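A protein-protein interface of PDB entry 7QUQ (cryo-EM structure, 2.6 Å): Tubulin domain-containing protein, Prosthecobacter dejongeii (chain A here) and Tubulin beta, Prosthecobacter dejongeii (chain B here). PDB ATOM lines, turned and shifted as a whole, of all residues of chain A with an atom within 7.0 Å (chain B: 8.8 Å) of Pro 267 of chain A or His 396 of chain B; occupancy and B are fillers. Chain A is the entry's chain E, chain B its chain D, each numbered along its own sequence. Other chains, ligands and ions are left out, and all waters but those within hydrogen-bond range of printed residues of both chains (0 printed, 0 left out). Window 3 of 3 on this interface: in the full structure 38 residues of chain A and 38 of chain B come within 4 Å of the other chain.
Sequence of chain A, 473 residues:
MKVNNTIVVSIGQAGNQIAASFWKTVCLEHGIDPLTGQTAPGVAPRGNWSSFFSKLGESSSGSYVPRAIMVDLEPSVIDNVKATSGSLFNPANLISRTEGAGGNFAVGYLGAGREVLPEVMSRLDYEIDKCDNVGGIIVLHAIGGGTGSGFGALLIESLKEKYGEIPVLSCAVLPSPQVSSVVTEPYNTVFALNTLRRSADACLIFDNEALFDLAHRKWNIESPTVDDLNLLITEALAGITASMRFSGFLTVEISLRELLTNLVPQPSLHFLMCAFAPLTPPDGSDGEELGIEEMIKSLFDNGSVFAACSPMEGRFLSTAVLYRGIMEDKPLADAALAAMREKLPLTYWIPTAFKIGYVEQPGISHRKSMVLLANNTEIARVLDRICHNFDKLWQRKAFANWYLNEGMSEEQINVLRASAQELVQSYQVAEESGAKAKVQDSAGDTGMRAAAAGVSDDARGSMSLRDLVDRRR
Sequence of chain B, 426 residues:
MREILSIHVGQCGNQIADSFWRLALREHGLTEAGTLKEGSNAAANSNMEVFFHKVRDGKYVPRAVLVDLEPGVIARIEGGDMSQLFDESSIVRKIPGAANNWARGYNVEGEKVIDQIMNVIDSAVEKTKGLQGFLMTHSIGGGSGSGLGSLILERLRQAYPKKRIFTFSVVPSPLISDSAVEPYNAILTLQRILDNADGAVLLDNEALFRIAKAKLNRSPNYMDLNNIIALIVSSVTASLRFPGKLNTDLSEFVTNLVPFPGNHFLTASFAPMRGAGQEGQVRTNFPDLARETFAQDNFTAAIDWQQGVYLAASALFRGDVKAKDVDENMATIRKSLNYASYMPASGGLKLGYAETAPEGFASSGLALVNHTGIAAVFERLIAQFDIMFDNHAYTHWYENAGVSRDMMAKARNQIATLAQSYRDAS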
ATOM      1  N   LEU A 196      -6.670 -25.767  13.657  1.00  0.00           N
ATOM      2  CA  LEU A 196      -5.357 -25.257  14.033  1.00  0.00           C
ATOM      3  C   LEU A 196      -4.931 -24.118  13.121  1.00  0.00           C
ATOM      4  O   LEU A 196      -4.384 -23.112  13.585  1.00  0.00           O
ATOM      5  CB  LEU A 196      -4.325 -26.385  13.999  1.00  0.00           C
ATOM      6  CG  LEU A 196      -4.403 -27.429  15.114  1.00  0.00           C
ATOM      7  CD1 LEU A 196      -3.333 -28.494  14.939  1.00  0.00           C
ATOM      8  CD2 LEU A 196      -4.284 -26.764  16.471  1.00  0.00           C
ATOM      9  N   ARG A 197      -5.182 -24.251  11.817  1.00  0.00           N
ATOM     10  CA  ARG A 197      -4.856 -23.156  10.909  1.00  0.00           C
ATOM     11  C   ARG A 197      -5.811 -21.988  11.122  1.00  0.00           C
ATOM     12  O   ARG A 197      -5.408 -20.820  11.061  1.00  0.00           O
ATOM     13  CB  ARG A 197      -4.899 -23.639   9.455  1.00  0.00           C
ATOM     14  CG  ARG A 197      -4.426 -22.618   8.402  1.00  0.00           C
ATOM     15  CD  ARG A 197      -5.499 -21.656   7.891  1.00  0.00           C
ATOM     16  NE  ARG A 197      -6.659 -22.331   7.327  1.00  0.00           N
ATOM     17  CZ  ARG A 197      -6.719 -22.803   6.089  1.00  0.00           C
ATOM     18  NH1 ARG A 197      -5.685 -22.723   5.268  1.00  0.00           N
ATOM     19  NH2 ARG A 197      -7.847 -23.358   5.661  1.00  0.00           N
ATOM     20  N   ALA A 200      -5.545 -21.490  15.931  1.00  0.00           N
ATOM     21  CA  ALA A 200      -4.270 -21.440  16.635  1.00  0.00           C
ATOM     22  C   ALA A 200      -3.277 -20.561  15.887  1.00  0.00           C
ATOM     23  O   ALA A 200      -3.128 -20.671  14.665  1.00  0.00           O
ATOM     24  CB  ALA A 200      -3.706 -22.848  16.808  1.00  0.00           C
ATOM     25  N   ASP A 201      -2.596 -19.682  16.624  1.00  0.00           N
ATOM     26  CA  ASP A 201      -1.556 -18.848  16.038  1.00  0.00           C
ATOM     27  C   ASP A 201      -0.223 -19.566  15.902  1.00  0.00           C
ATOM     28  O   ASP A 201       0.684 -19.024  15.265  1.00  0.00           O
ATOM     29  CB  ASP A 201      -1.371 -17.569  16.856  1.00  0.00           C
ATOM     30  CG  ASP A 201      -2.683 -16.883  17.164  1.00  0.00           C
ATOM     31  OD1 ASP A 201      -3.643 -17.085  16.392  1.00  0.00           O
ATOM     32  OD2 ASP A 201      -2.754 -16.139  18.162  1.00  0.00           O
ATOM     33  N   LEU A 260       6.280 -16.155  18.854  1.00  0.00           N
ATOM     34  CA  LEU A 260       5.296 -16.187  17.781  1.00  0.00           C
ATOM     35  C   LEU A 260       5.688 -15.244  16.652  1.00  0.00           C
ATOM     36  O   LEU A 260       5.711 -15.632  15.479  1.00  0.00           O
ATOM     37  CB  LEU A 260       3.929 -15.803  18.346  1.00  0.00           C
ATOM     38  CG  LEU A 260       2.675 -16.165  17.561  1.00  0.00           C
ATOM     39  CD1 LEU A 260       2.501 -17.648  17.572  1.00  0.00           C
ATOM     40  CD2 LEU A 260       1.463 -15.481  18.156  1.00  0.00           C
ATOM     41  N   THR A 261       6.003 -13.995  16.998  1.00  0.00           N
ATOM     42  CA  THR A 261       6.362 -12.998  16.000  1.00  0.00           C
ATOM     43  C   THR A 261       7.636 -13.395  15.271  1.00  0.00           C
ATOM     44  O   THR A 261       7.751 -13.206  14.055  1.00  0.00           O
ATOM     45  CB  THR A 261       6.511 -11.628  16.669  1.00  0.00           C
ATOM     46  OG1 THR A 261       5.215 -11.104  16.976  1.00  0.00           O
ATOM     47  CG2 THR A 261       7.240 -10.641  15.766  1.00  0.00           C
ATOM     48  N   VAL A 264       6.489 -17.045  13.288  1.00  0.00           N
ATOM     49  CA  VAL A 264       5.330 -17.077  12.409  1.00  0.00           C
ATOM     50  C   VAL A 264       5.415 -15.878  11.473  1.00  0.00           C
ATOM     51  O   VAL A 264       4.992 -14.775  11.817  1.00  0.00           O
ATOM     52  CB  VAL A 264       4.014 -17.068  13.208  1.00  0.00           C
ATOM     53  CG1 VAL A 264       2.814 -17.112  12.278  1.00  0.00           C
ATOM     54  CG2 VAL A 264       3.984 -18.229  14.190  1.00  0.00           C
ATOM     55  N   PRO A 265       5.985 -16.052  10.279  1.00  0.00           N
ATOM     56  CA  PRO A 265       6.032 -14.940   9.322  1.00  0.00           C
ATOM     57  C   PRO A 265       4.663 -14.604   8.748  1.00  0.00           C
ATOM     58  O   PRO A 265       4.243 -13.444   8.765  1.00  0.00           O
ATOM     59  CB  PRO A 265       6.994 -15.449   8.239  1.00  0.00           C
ATOM     60  CG  PRO A 265       6.961 -16.928   8.347  1.00  0.00           C
ATOM     61  CD  PRO A 265       6.652 -17.265   9.773  1.00  0.00           C
ATOM     62  N   GLN A 266       3.940 -15.614   8.273  1.00  0.00           N
ATOM     63  CA  GLN A 266       2.651 -15.411   7.640  1.00  0.00           C
ATOM     64  C   GLN A 266       1.552 -16.054   8.478  1.00  0.00           C
ATOM     65  O   GLN A 266       1.819 -17.003   9.222  1.00  0.00           O
ATOM     66  CB  GLN A 266       2.643 -15.994   6.220  1.00  0.00           C
ATOM     67  CG  GLN A 266       3.695 -15.378   5.308  1.00  0.00           C
ATOM     68  CD  GLN A 266       3.765 -16.046   3.951  1.00  0.00           C
ATOM     69  OE1 GLN A 266       2.903 -16.851   3.596  1.00  0.00           O
ATOM     70  NE2 GLN A 266       4.796 -15.717   3.181  1.00  0.00           N
ATOM     71  N   PRO A 267       0.314 -15.550   8.394  1.00  0.00           N
ATOM     72  CA  PRO A 267      -0.751 -16.079   9.266  1.00  0.00           C
ATOM     73  C   PRO A 267      -1.010 -17.567   9.101  1.00  0.00           C
ATOM     74  O   PRO A 267      -1.401 -18.227  10.071  1.00  0.00           O
ATOM     75  CB  PRO A 267      -1.975 -15.248   8.857  1.00  0.00           C
ATOM     76  CG  PRO A 267      -1.403 -13.983   8.324  1.00  0.00           C
ATOM     77  CD  PRO A 267      -0.143 -14.383   7.619  1.00  0.00           C
ATOM     78  N   SER A 268      -0.802 -18.118   7.909  1.00  0.00           N
ATOM     79  CA  SER A 268      -0.980 -19.544   7.681  1.00  0.00           C
ATOM     80  C   SER A 268       0.290 -20.350   7.919  1.00  0.00           C
ATOM     81  O   SER A 268       0.230 -21.585   7.927  1.00  0.00           O
ATOM     82  CB  SER A 268      -1.483 -19.792   6.254  1.00  0.00           C
ATOM     83  OG  SER A 268      -2.817 -19.335   6.100  1.00  0.00           O
ATOM     84  N   LEU A 269       1.431 -19.692   8.114  1.00  0.00           N
ATOM     85  CA  LEU A 269       2.703 -20.386   8.319  1.00  0.00           C
ATOM     86  C   LEU A 269       3.074 -20.348   9.801  1.00  0.00           C
ATOM     87  O   LEU A 269       3.855 -19.515  10.260  1.00  0.00           O
ATOM     88  CB  LEU A 269       3.791 -19.757   7.455  1.00  0.00           C
ATOM     89  CG  LEU A 269       3.639 -19.880   5.939  1.00  0.00           C
ATOM     90  CD1 LEU A 269       4.721 -19.089   5.229  1.00  0.00           C
ATOM     91  CD2 LEU A 269       3.670 -21.328   5.504  1.00  0.00           C
ATOM     92  N   HIS A 270       2.496 -21.284  10.558  1.00  0.00           N
ATOM     93  CA  HIS A 270       2.706 -21.287  12.000  1.00  0.00           C
ATOM     94  C   HIS A 270       2.852 -22.696  12.567  1.00  0.00           C
ATOM     95  O   HIS A 270       2.486 -22.944  13.720  1.00  0.00           O
ATOM     96  CB  HIS A 270       1.568 -20.560  12.712  1.00  0.00           C
ATOM     97  CG  HIS A 270       0.217 -21.156  12.467  1.00  0.00           C
ATOM     98  ND1 HIS A 270      -0.292 -22.183  13.231  1.00  0.00           N
ATOM     99  CD2 HIS A 270      -0.732 -20.866  11.546  1.00  0.00           C
ATOM    100  CE1 HIS A 270      -1.496 -22.502  12.790  1.00  0.00           C
ATOM    101  NE2 HIS A 270      -1.786 -21.718  11.768  1.00  0.00           N
ATOM    102  N   ASN B 101       7.917  -6.550  18.012  1.00  0.00           N
ATOM    103  CA  ASN B 101       7.171  -5.720  17.080  1.00  0.00           C
ATOM    104  C   ASN B 101       7.386  -4.249  17.411  1.00  0.00           C
ATOM    105  O   ASN B 101       7.238  -3.838  18.565  1.00  0.00           O
ATOM    106  CB  ASN B 101       5.683  -6.066  17.128  1.00  0.00           C
ATOM    107  CG  ASN B 101       5.033  -6.035  15.765  1.00  0.00           C
ATOM    108  OD1 ASN B 101       5.671  -6.329  14.757  1.00  0.00           O
ATOM    109  ND2 ASN B 101       3.751  -5.690  15.726  1.00  0.00           N
ATOM    110  N   ALA B 103       5.443  -1.866  16.219  1.00  0.00           N
ATOM    111  CA  ALA B 103       4.108  -1.354  16.503  1.00  0.00           C
ATOM    112  C   ALA B 103       3.655  -1.713  17.909  1.00  0.00           C
ATOM    113  O   ALA B 103       2.915  -0.947  18.534  1.00  0.00           O
ATOM    114  CB  ALA B 103       3.116  -1.893  15.478  1.00  0.00           C
ATOM    115  N   ARG B 104       4.083  -2.869  18.418  1.00  0.00           N
ATOM    116  CA  ARG B 104       3.682  -3.276  19.758  1.00  0.00           C
ATOM    117  C   ARG B 104       4.301  -2.376  20.820  1.00  0.00           C
ATOM    118  O   ARG B 104       3.727  -2.204  21.900  1.00  0.00           O
ATOM    119  CB  ARG B 104       4.061  -4.737  19.985  1.00  0.00           C
ATOM    120  CG  ARG B 104       3.487  -5.359  21.233  1.00  0.00           C
ATOM    121  CD  ARG B 104       3.454  -6.872  21.104  1.00  0.00           C
ATOM    122  NE  ARG B 104       2.883  -7.301  19.833  1.00  0.00           N
ATOM    123  CZ  ARG B 104       1.582  -7.388  19.587  1.00  0.00           C
ATOM    124  NH1 ARG B 104       0.683  -7.069  20.502  1.00  0.00           N
ATOM    125  NH2 ARG B 104       1.175  -7.807  18.392  1.00  0.00           N
ATOM    126  N   VAL B 181      12.508 -10.385  13.079  1.00  0.00           N
ATOM    127  CA  VAL B 181      11.832  -9.233  12.494  1.00  0.00           C
ATOM    128  C   VAL B 181      12.636  -7.953  12.697  1.00  0.00           C
ATOM    129  O   VAL B 181      12.122  -6.850  12.462  1.00  0.00           O
ATOM    130  CB  VAL B 181      10.402  -9.159  13.077  1.00  0.00           C
ATOM    131  CG1 VAL B 181      10.422  -8.636  14.495  1.00  0.00           C
ATOM    132  CG2 VAL B 181       9.461  -8.357  12.181  1.00  0.00           C
ATOM    133  N   TYR B 184      12.907  -4.753  10.060  1.00  0.00           N
ATOM    134  CA  TYR B 184      11.763  -3.856  10.198  1.00  0.00           C
ATOM    135  C   TYR B 184      11.959  -2.901  11.365  1.00  0.00           C
ATOM    136  O   TYR B 184      11.822  -1.680  11.217  1.00  0.00           O
ATOM    137  CB  TYR B 184      10.479  -4.662  10.401  1.00  0.00           C
ATOM    138  CG  TYR B 184       9.961  -5.383   9.181  1.00  0.00           C
ATOM    139  CD1 TYR B 184      10.421  -5.069   7.913  1.00  0.00           C
ATOM    140  CD2 TYR B 184       8.983  -6.362   9.298  1.00  0.00           C
ATOM    141  CE1 TYR B 184       9.932  -5.718   6.798  1.00  0.00           C
ATOM    142  CE2 TYR B 184       8.492  -7.019   8.191  1.00  0.00           C
ATOM    143  CZ  TYR B 184       8.965  -6.689   6.943  1.00  0.00           C
ATOM    144  OH  TYR B 184       8.484  -7.340   5.832  1.00  0.00           O
ATOM    145  N   PHE B 389      10.494  -7.176   2.872  1.00  0.00           N
ATOM    146  CA  PHE B 389       9.245  -6.465   2.614  1.00  0.00           C
ATOM    147  C   PHE B 389       8.546  -6.978   1.363  1.00  0.00           C
ATOM    148  O   PHE B 389       7.326  -7.185   1.366  1.00  0.00           O
ATOM    149  CB  PHE B 389       9.519  -4.971   2.492  1.00  0.00           C
ATOM    150  CG  PHE B 389       8.294  -4.113   2.621  1.00  0.00           C
ATOM    151  CD1 PHE B 389       7.639  -3.990   3.834  1.00  0.00           C
ATOM    152  CD2 PHE B 389       7.816  -3.403   1.532  1.00  0.00           C
ATOM    153  CE1 PHE B 389       6.520  -3.192   3.954  1.00  0.00           C
ATOM    154  CE2 PHE B 389       6.698  -2.601   1.648  1.00  0.00           C
ATOM    155  CZ  PHE B 389       6.049  -2.497   2.859  1.00  0.00           C
ATOM    156  N   HIS B 392       6.265 -10.047   1.734  1.00  0.00           N
ATOM    157  CA  HIS B 392       5.243  -9.984   2.781  1.00  0.00           C
ATOM    158  C   HIS B 392       5.636 -10.858   3.973  1.00  0.00           C
ATOM    159  O   HIS B 392       4.848 -11.654   4.487  1.00  0.00           O
ATOM    160  CB  HIS B 392       3.867 -10.381   2.237  1.00  0.00           C
ATOM    161  CG  HIS B 392       3.088  -9.239   1.666  1.00  0.00           C
ATOM    162  ND1 HIS B 392       2.092  -8.594   2.366  1.00  0.00           N
ATOM    163  CD2 HIS B 392       3.153  -8.631   0.458  1.00  0.00           C
ATOM    164  CE1 HIS B 392       1.579  -7.635   1.616  1.00  0.00           C
ATOM    165  NE2 HIS B 392       2.205  -7.636   0.453  1.00  0.00           N
ATOM    166  N   ALA B 393       6.888 -10.697   4.402  1.00  0.00           N
ATOM    167  CA  ALA B 393       7.479 -11.629   5.353  1.00  0.00           C
ATOM    168  C   ALA B 393       6.810 -11.566   6.716  1.00  0.00           C
ATOM    169  O   ALA B 393       6.216 -12.554   7.149  1.00  0.00           O
ATOM    170  CB  ALA B 393       8.979 -11.378   5.499  1.00  0.00           C
ATOM    171  N   TYR B 394       6.883 -10.427   7.401  1.00  0.00           N
ATOM    172  CA  TYR B 394       6.320 -10.311   8.739  1.00  0.00           C
ATOM    173  C   TYR B 394       5.398  -9.101   8.852  1.00  0.00           C
ATOM    174  O   TYR B 394       5.131  -8.616   9.953  1.00  0.00           O
ATOM    175  CB  TYR B 394       7.421 -10.231   9.796  1.00  0.00           C
ATOM    176  CG  TYR B 394       8.224 -11.503   9.973  1.00  0.00           C
ATOM    177  CD1 TYR B 394       9.170 -11.885   9.034  1.00  0.00           C
ATOM    178  CD2 TYR B 394       8.018 -12.332  11.065  1.00  0.00           C
ATOM    179  CE1 TYR B 394       9.902 -13.042   9.187  1.00  0.00           C
ATOM    180  CE2 TYR B 394       8.748 -13.499  11.221  1.00  0.00           C
ATOM    181  CZ  TYR B 394       9.685 -13.848  10.280  1.00  0.00           C
ATOM    182  OH  TYR B 394      10.412 -15.007  10.433  1.00  0.00           O
ATOM    183  N   THR B 395       4.904  -8.608   7.716  1.00  0.00           N
ATOM    184  CA  THR B 395       4.148  -7.361   7.695  1.00  0.00           C
ATOM    185  C   THR B 395       2.787  -7.464   8.369  1.00  0.00           C
ATOM    186  O   THR B 395       2.246  -6.432   8.776  1.00  0.00           O
ATOM    187  CB  THR B 395       3.967  -6.880   6.256  1.00  0.00           C
ATOM    188  OG1 THR B 395       3.251  -7.870   5.504  1.00  0.00           O
ATOM    189  CG2 THR B 395       5.318  -6.632   5.612  1.00  0.00           C
ATOM    190  N   HIS B 396       2.219  -8.666   8.495  1.00  0.00           N
ATOM    191  CA  HIS B 396       0.926  -8.778   9.161  1.00  0.00           C
ATOM    192  C   HIS B 396       1.046  -8.496  10.653  1.00  0.00           C
ATOM    193  O   HIS B 396       0.108  -7.966  11.256  1.00  0.00           O
ATOM    194  CB  HIS B 396       0.310 -10.157   8.920  1.00  0.00           C
ATOM    195  CG  HIS B 396       0.772 -11.207   9.880  1.00  0.00           C
ATOM    196  ND1 HIS B 396       0.101 -11.493  11.050  1.00  0.00           N
ATOM    197  CD2 HIS B 396       1.834 -12.045   9.843  1.00  0.00           C
ATOM    198  CE1 HIS B 396       0.733 -12.459  11.693  1.00  0.00           C
ATOM    199  NE2 HIS B 396       1.788 -12.812  10.980  1.00  0.00           N
ATOM    200  N   TRP B 397       2.200  -8.816  11.253  1.00  0.00           N
ATOM    201  CA  TRP B 397       2.426  -8.532  12.666  1.00  0.00           C
ATOM    202  C   TRP B 397       2.349  -7.048  12.976  1.00  0.00           C
ATOM    203  O   TRP B 397       2.032  -6.677  14.111  1.00  0.00           O
ATOM    204  CB  TRP B 397       3.788  -9.071  13.104  1.00  0.00           C
ATOM    205  CG  TRP B 397       3.857 -10.556  13.138  1.00  0.00           C
ATOM    206  CD1 TRP B 397       4.647 -11.359  12.370  1.00  0.00           C
ATOM    207  CD2 TRP B 397       3.090 -11.426  13.975  1.00  0.00           C
ATOM    208  NE1 TRP B 397       4.425 -12.677  12.684  1.00  0.00           N
ATOM    209  CE2 TRP B 397       3.474 -12.744  13.666  1.00  0.00           C
ATOM    210  CE3 TRP B 397       2.119 -11.218  14.958  1.00  0.00           C
ATOM    211  CZ2 TRP B 397       2.920 -13.847  14.304  1.00  0.00           C
ATOM    212  CZ3 TRP B 397       1.573 -12.313  15.589  1.00  0.00           C
ATOM    213  CH2 TRP B 397       1.972 -13.610  15.259  1.00  0.00           C
ATOM    214  N   TYR B 398       2.643  -6.196  11.998  1.00  0.00           N
ATOM    215  CA  TYR B 398       2.519  -4.755  12.156  1.00  0.00           C
ATOM    216  C   TYR B 398       1.152  -4.265  11.696  1.00  0.00           C
ATOM    217  O   TYR B 398       0.558  -3.386  12.330  1.00  0.00           O
ATOM    218  CB  TYR B 398       3.628  -4.051  11.367  1.00  0.00           C
ATOM    219  CG  TYR B 398       5.017  -4.342  11.878  1.00  0.00           C
ATOM    220  CD1 TYR B 398       5.649  -3.478  12.759  1.00  0.00           C
ATOM    221  CD2 TYR B 398       5.698  -5.484  11.480  1.00  0.00           C
ATOM    222  CE1 TYR B 398       6.918  -3.744  13.227  1.00  0.00           C
ATOM    223  CE2 TYR B 398       6.966  -5.758  11.944  1.00  0.00           C
ATOM    224  CZ  TYR B 398       7.573  -4.884  12.817  1.00  0.00           C
ATOM    225  OH  TYR B 398       8.839  -5.154  13.283  1.00  0.00           O
ATOM    226  N   GLU B 399       0.649  -4.824  10.589  1.00  0.00           N
ATOM    227  CA  GLU B 399      -0.628  -4.388  10.036  1.00  0.00           C
ATOM    228  C   GLU B 399      -1.783  -4.653  10.991  1.00  0.00           C
ATOM    229  O   GLU B 399      -2.655  -3.791  11.158  1.00  0.00           O
ATOM    230  CB  GLU B 399      -0.880  -5.077   8.696  1.00  0.00           C
ATOM    231  CG  GLU B 399      -0.076  -4.501   7.544  1.00  0.00           C
ATOM    232  CD  GLU B 399      -0.841  -4.519   6.234  1.00  0.00           C
ATOM    233  OE1 GLU B 399      -1.195  -5.623   5.766  1.00  0.00           O
ATOM    234  OE2 GLU B 399      -1.082  -3.430   5.671  1.00  0.00           O
ATOM    235  N   ASN B 400      -1.813  -5.825  11.626  1.00  0.00           N
ATOM    236  CA  ASN B 400      -2.821  -6.104  12.637  1.00  0.00           C
ATOM    237  C   ASN B 400      -2.561  -5.358  13.937  1.00  0.00           C
ATOM    238  O   ASN B 400      -3.450  -5.306  14.792  1.00  0.00           O
ATOM    239  CB  ASN B 400      -2.889  -7.609  12.909  1.00  0.00           C
ATOM    240  CG  ASN B 400      -3.225  -8.408  11.665  1.00  0.00           C
ATOM    241  OD1 ASN B 400      -4.057  -7.998  10.855  1.00  0.00           O
ATOM    242  ND2 ASN B 400      -2.578  -9.556  11.505  1.00  0.00           N
ATOM    243  N   ALA B 401      -1.372  -4.785  14.098  1.00  0.00           N
ATOM    244  CA  ALA B 401      -1.023  -4.009  15.277  1.00  0.00           C
ATOM    245  C   ALA B 401      -1.229  -2.511  15.085  1.00  0.00           C
ATOM    246  O   ALA B 401      -1.055  -1.750  16.042  1.00  0.00           O
ATOM    247  CB  ALA B 401       0.428  -4.289  15.672  1.00  0.00           C
ATOM    248  N   GLY B 402      -1.594  -2.070  13.882  1.00  0.00           N
ATOM    249  CA  GLY B 402      -1.893  -0.676  13.619  1.00  0.00           C
ATOM    250  C   GLY B 402      -0.892   0.052  12.747  1.00  0.00           C
ATOM    251  O   GLY B 402      -1.184   1.173  12.311  1.00  0.00           O
ATOM    252  N   VAL B 403       0.272  -0.532  12.473  1.00  0.00           N
ATOM    253  CA  VAL B 403       1.286   0.083  11.623  1.00  0.00           C
ATOM    254  C   VAL B 403       1.224  -0.609  10.267  1.00  0.00           C
ATOM    255  O   VAL B 403       1.605  -1.778  10.134  1.00  0.00           O
ATOM    256  CB  VAL B 403       2.685  -0.004  12.248  1.00  0.00           C
ATOM    257  CG1 VAL B 403       3.768   0.251  11.210  1.00  0.00           C
ATOM    258  CG2 VAL B 403       2.807   0.999  13.381  1.00  0.00           C
ATOM    259  N   SER B 404       0.740   0.108   9.258  1.00  0.00           N
ATOM    260  CA  SER B 404       0.534  -0.480   7.945  1.00  0.00           C
ATOM    261  C   SER B 404       1.852  -0.556   7.177  1.00  0.00           C
ATOM    262  O   SER B 404       2.910  -0.128   7.647  1.00  0.00           O
ATOM    263  CB  SER B 404      -0.514   0.315   7.170  1.00  0.00           C
ATOM    264  OG  SER B 404      -0.258   1.707   7.244  1.00  0.00           O
ATOM    265  N   ARG B 405       1.782  -1.122   5.970  1.00  0.00           N
ATOM    266  CA  ARG B 405       2.979  -1.314   5.159  1.00  0.00           C
ATOM    267  C   ARG B 405       3.465  -0.006   4.545  1.00  0.00           C
ATOM    268  O   ARG B 405       4.651   0.119   4.221  1.00  0.00           O
ATOM    269  CB  ARG B 405       2.701  -2.346   4.065  1.00  0.00           C
ATOM    270  CG  ARG B 405       3.041  -3.772   4.464  1.00  0.00           C
ATOM    271  CD  ARG B 405       2.739  -4.765   3.350  1.00  0.00           C
ATOM    272  NE  ARG B 405       3.556  -4.568   2.159  1.00  0.00           N
ATOM    273  CZ  ARG B 405       4.459  -5.435   1.720  1.00  0.00           C
ATOM    274  NH1 ARG B 405       4.700  -6.565   2.364  1.00  0.00           N
ATOM    275  NH2 ARG B 405       5.127  -5.170   0.603  1.00  0.00           N
ATOM    276  N   MET B 408       5.849   1.922   6.889  1.00  0.00           N
ATOM    277  CA  MET B 408       7.107   1.183   6.872  1.00  0.00           C
ATOM    278  C   MET B 408       7.888   1.461   5.589  1.00  0.00           C
ATOM    279  O   MET B 408       9.114   1.648   5.619  1.00  0.00           O
ATOM    280  CB  MET B 408       6.818  -0.309   7.013  1.00  0.00           C
ATOM    281  CG  MET B 408       6.236  -0.691   8.359  1.00  0.00           C
ATOM    282  SD  MET B 408       5.834  -2.441   8.441  1.00  0.00           S
ATOM    283  CE  MET B 408       7.476  -3.142   8.472  1.00  0.00           C
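Pro 267 of chain A touches just one residue of chain B: His 396.
His 396 of chain B touches three residues of chain A.
Ser 268 of chain A touches none of the printed residues of chain B.
Printed residues of chain B within 4 Å of Gln 266 of chain A: His 392 (3.98 Å) and Ala 393 (3.98 Å).
Printed residues of chain A within 4 Å of Ala 393 of chain B: Pro 265 and Gln 266.
Of the printed residues of chain A, Trp 397 of chain B touches Leu 260, Thr 261, Val 264 and Pro 265.
Printed residues of chain B within 4 Å of Leu 260 of chain A: Trp 397.
The nearest residue of chain A that does not touch His 396 of chain B is Gln 266 of chain A (4.1 Å).
Hydrophobic or aromatic side chains of chain B that line the printed part of chain A: Val 181, Tyr 394, His 396 and Trp 397.
Hydrophobic or aromatic side chains of chain A within 4 Å of the printed part of chain B: Leu 260, Val 264, Pro 265 and Pro 267.
The side-chain amide nitrogen (ND2) of Asn 101 of chain B lies within hydrogen-bond range of the backbone carbonyl oxygen (O) of Trp 397 of chain B.
OG1 of Thr 395 of chain B sits at hydrogen-bond distance from ND1 of His 392 of chain B (3.4 Å).
The guanidinium group of Arg 405 of chain B lies close to a ring nitrogen (ND1) of His 392 of chain B (3.3 Å).
A ring nitrogen (NE2) of His 396 of chain B is in hydrogen-bond range of the indole nitrogen (NE1) of Trp 397 of chain B.
The backbone carbonyl oxygen (O) of His 396 of chain B is in hydrogen-bond range of the side-chain amide nitrogen (ND2) of Asn 400 of chain B (3.1 Å).
Among the printed residues, pairs that only touch across the chains: Thr 261 of chain A with Tyr 394 of chain B (3.0 Å), Leu 260 of chain A with Trp 397 of chain B (3.5 Å), Pro 265 of chain A with Tyr 394 of chain B (3.6 Å), Thr 261 of chain A with Trp 397 of chain B (3.6 Å), Pro 267 of chain A with His 396 of chain B (3.8 Å), Val 264 of chain A with His 396 of chain B (3.8 Å), Val 264 of chain A with Tyr 394 of chain B (3.96 Å), Thr 261 of chain A with Val 181 of chain B (3.97 Å), Gln 266 of chain A with Ala 393 of chain B (3.98 Å), Gln 266 of chain A with His 392 of chain B (3.98 Å) and Pro 265 of chain A with Trp 397 of chain B (3.997 Å).
The backbone carbonyl oxygen of Pro 265 of chain A lies close to the backbone carbonyl oxygen of Ala 393 of chain B (2.7 Å).
O of Pro 265 of chain A sits close to NE2 of His 396 of chain B, at 3.4 Å.
O of Val 264 of chain A lies close to NE1 of Trp 397 of chain B (2.3 Å).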
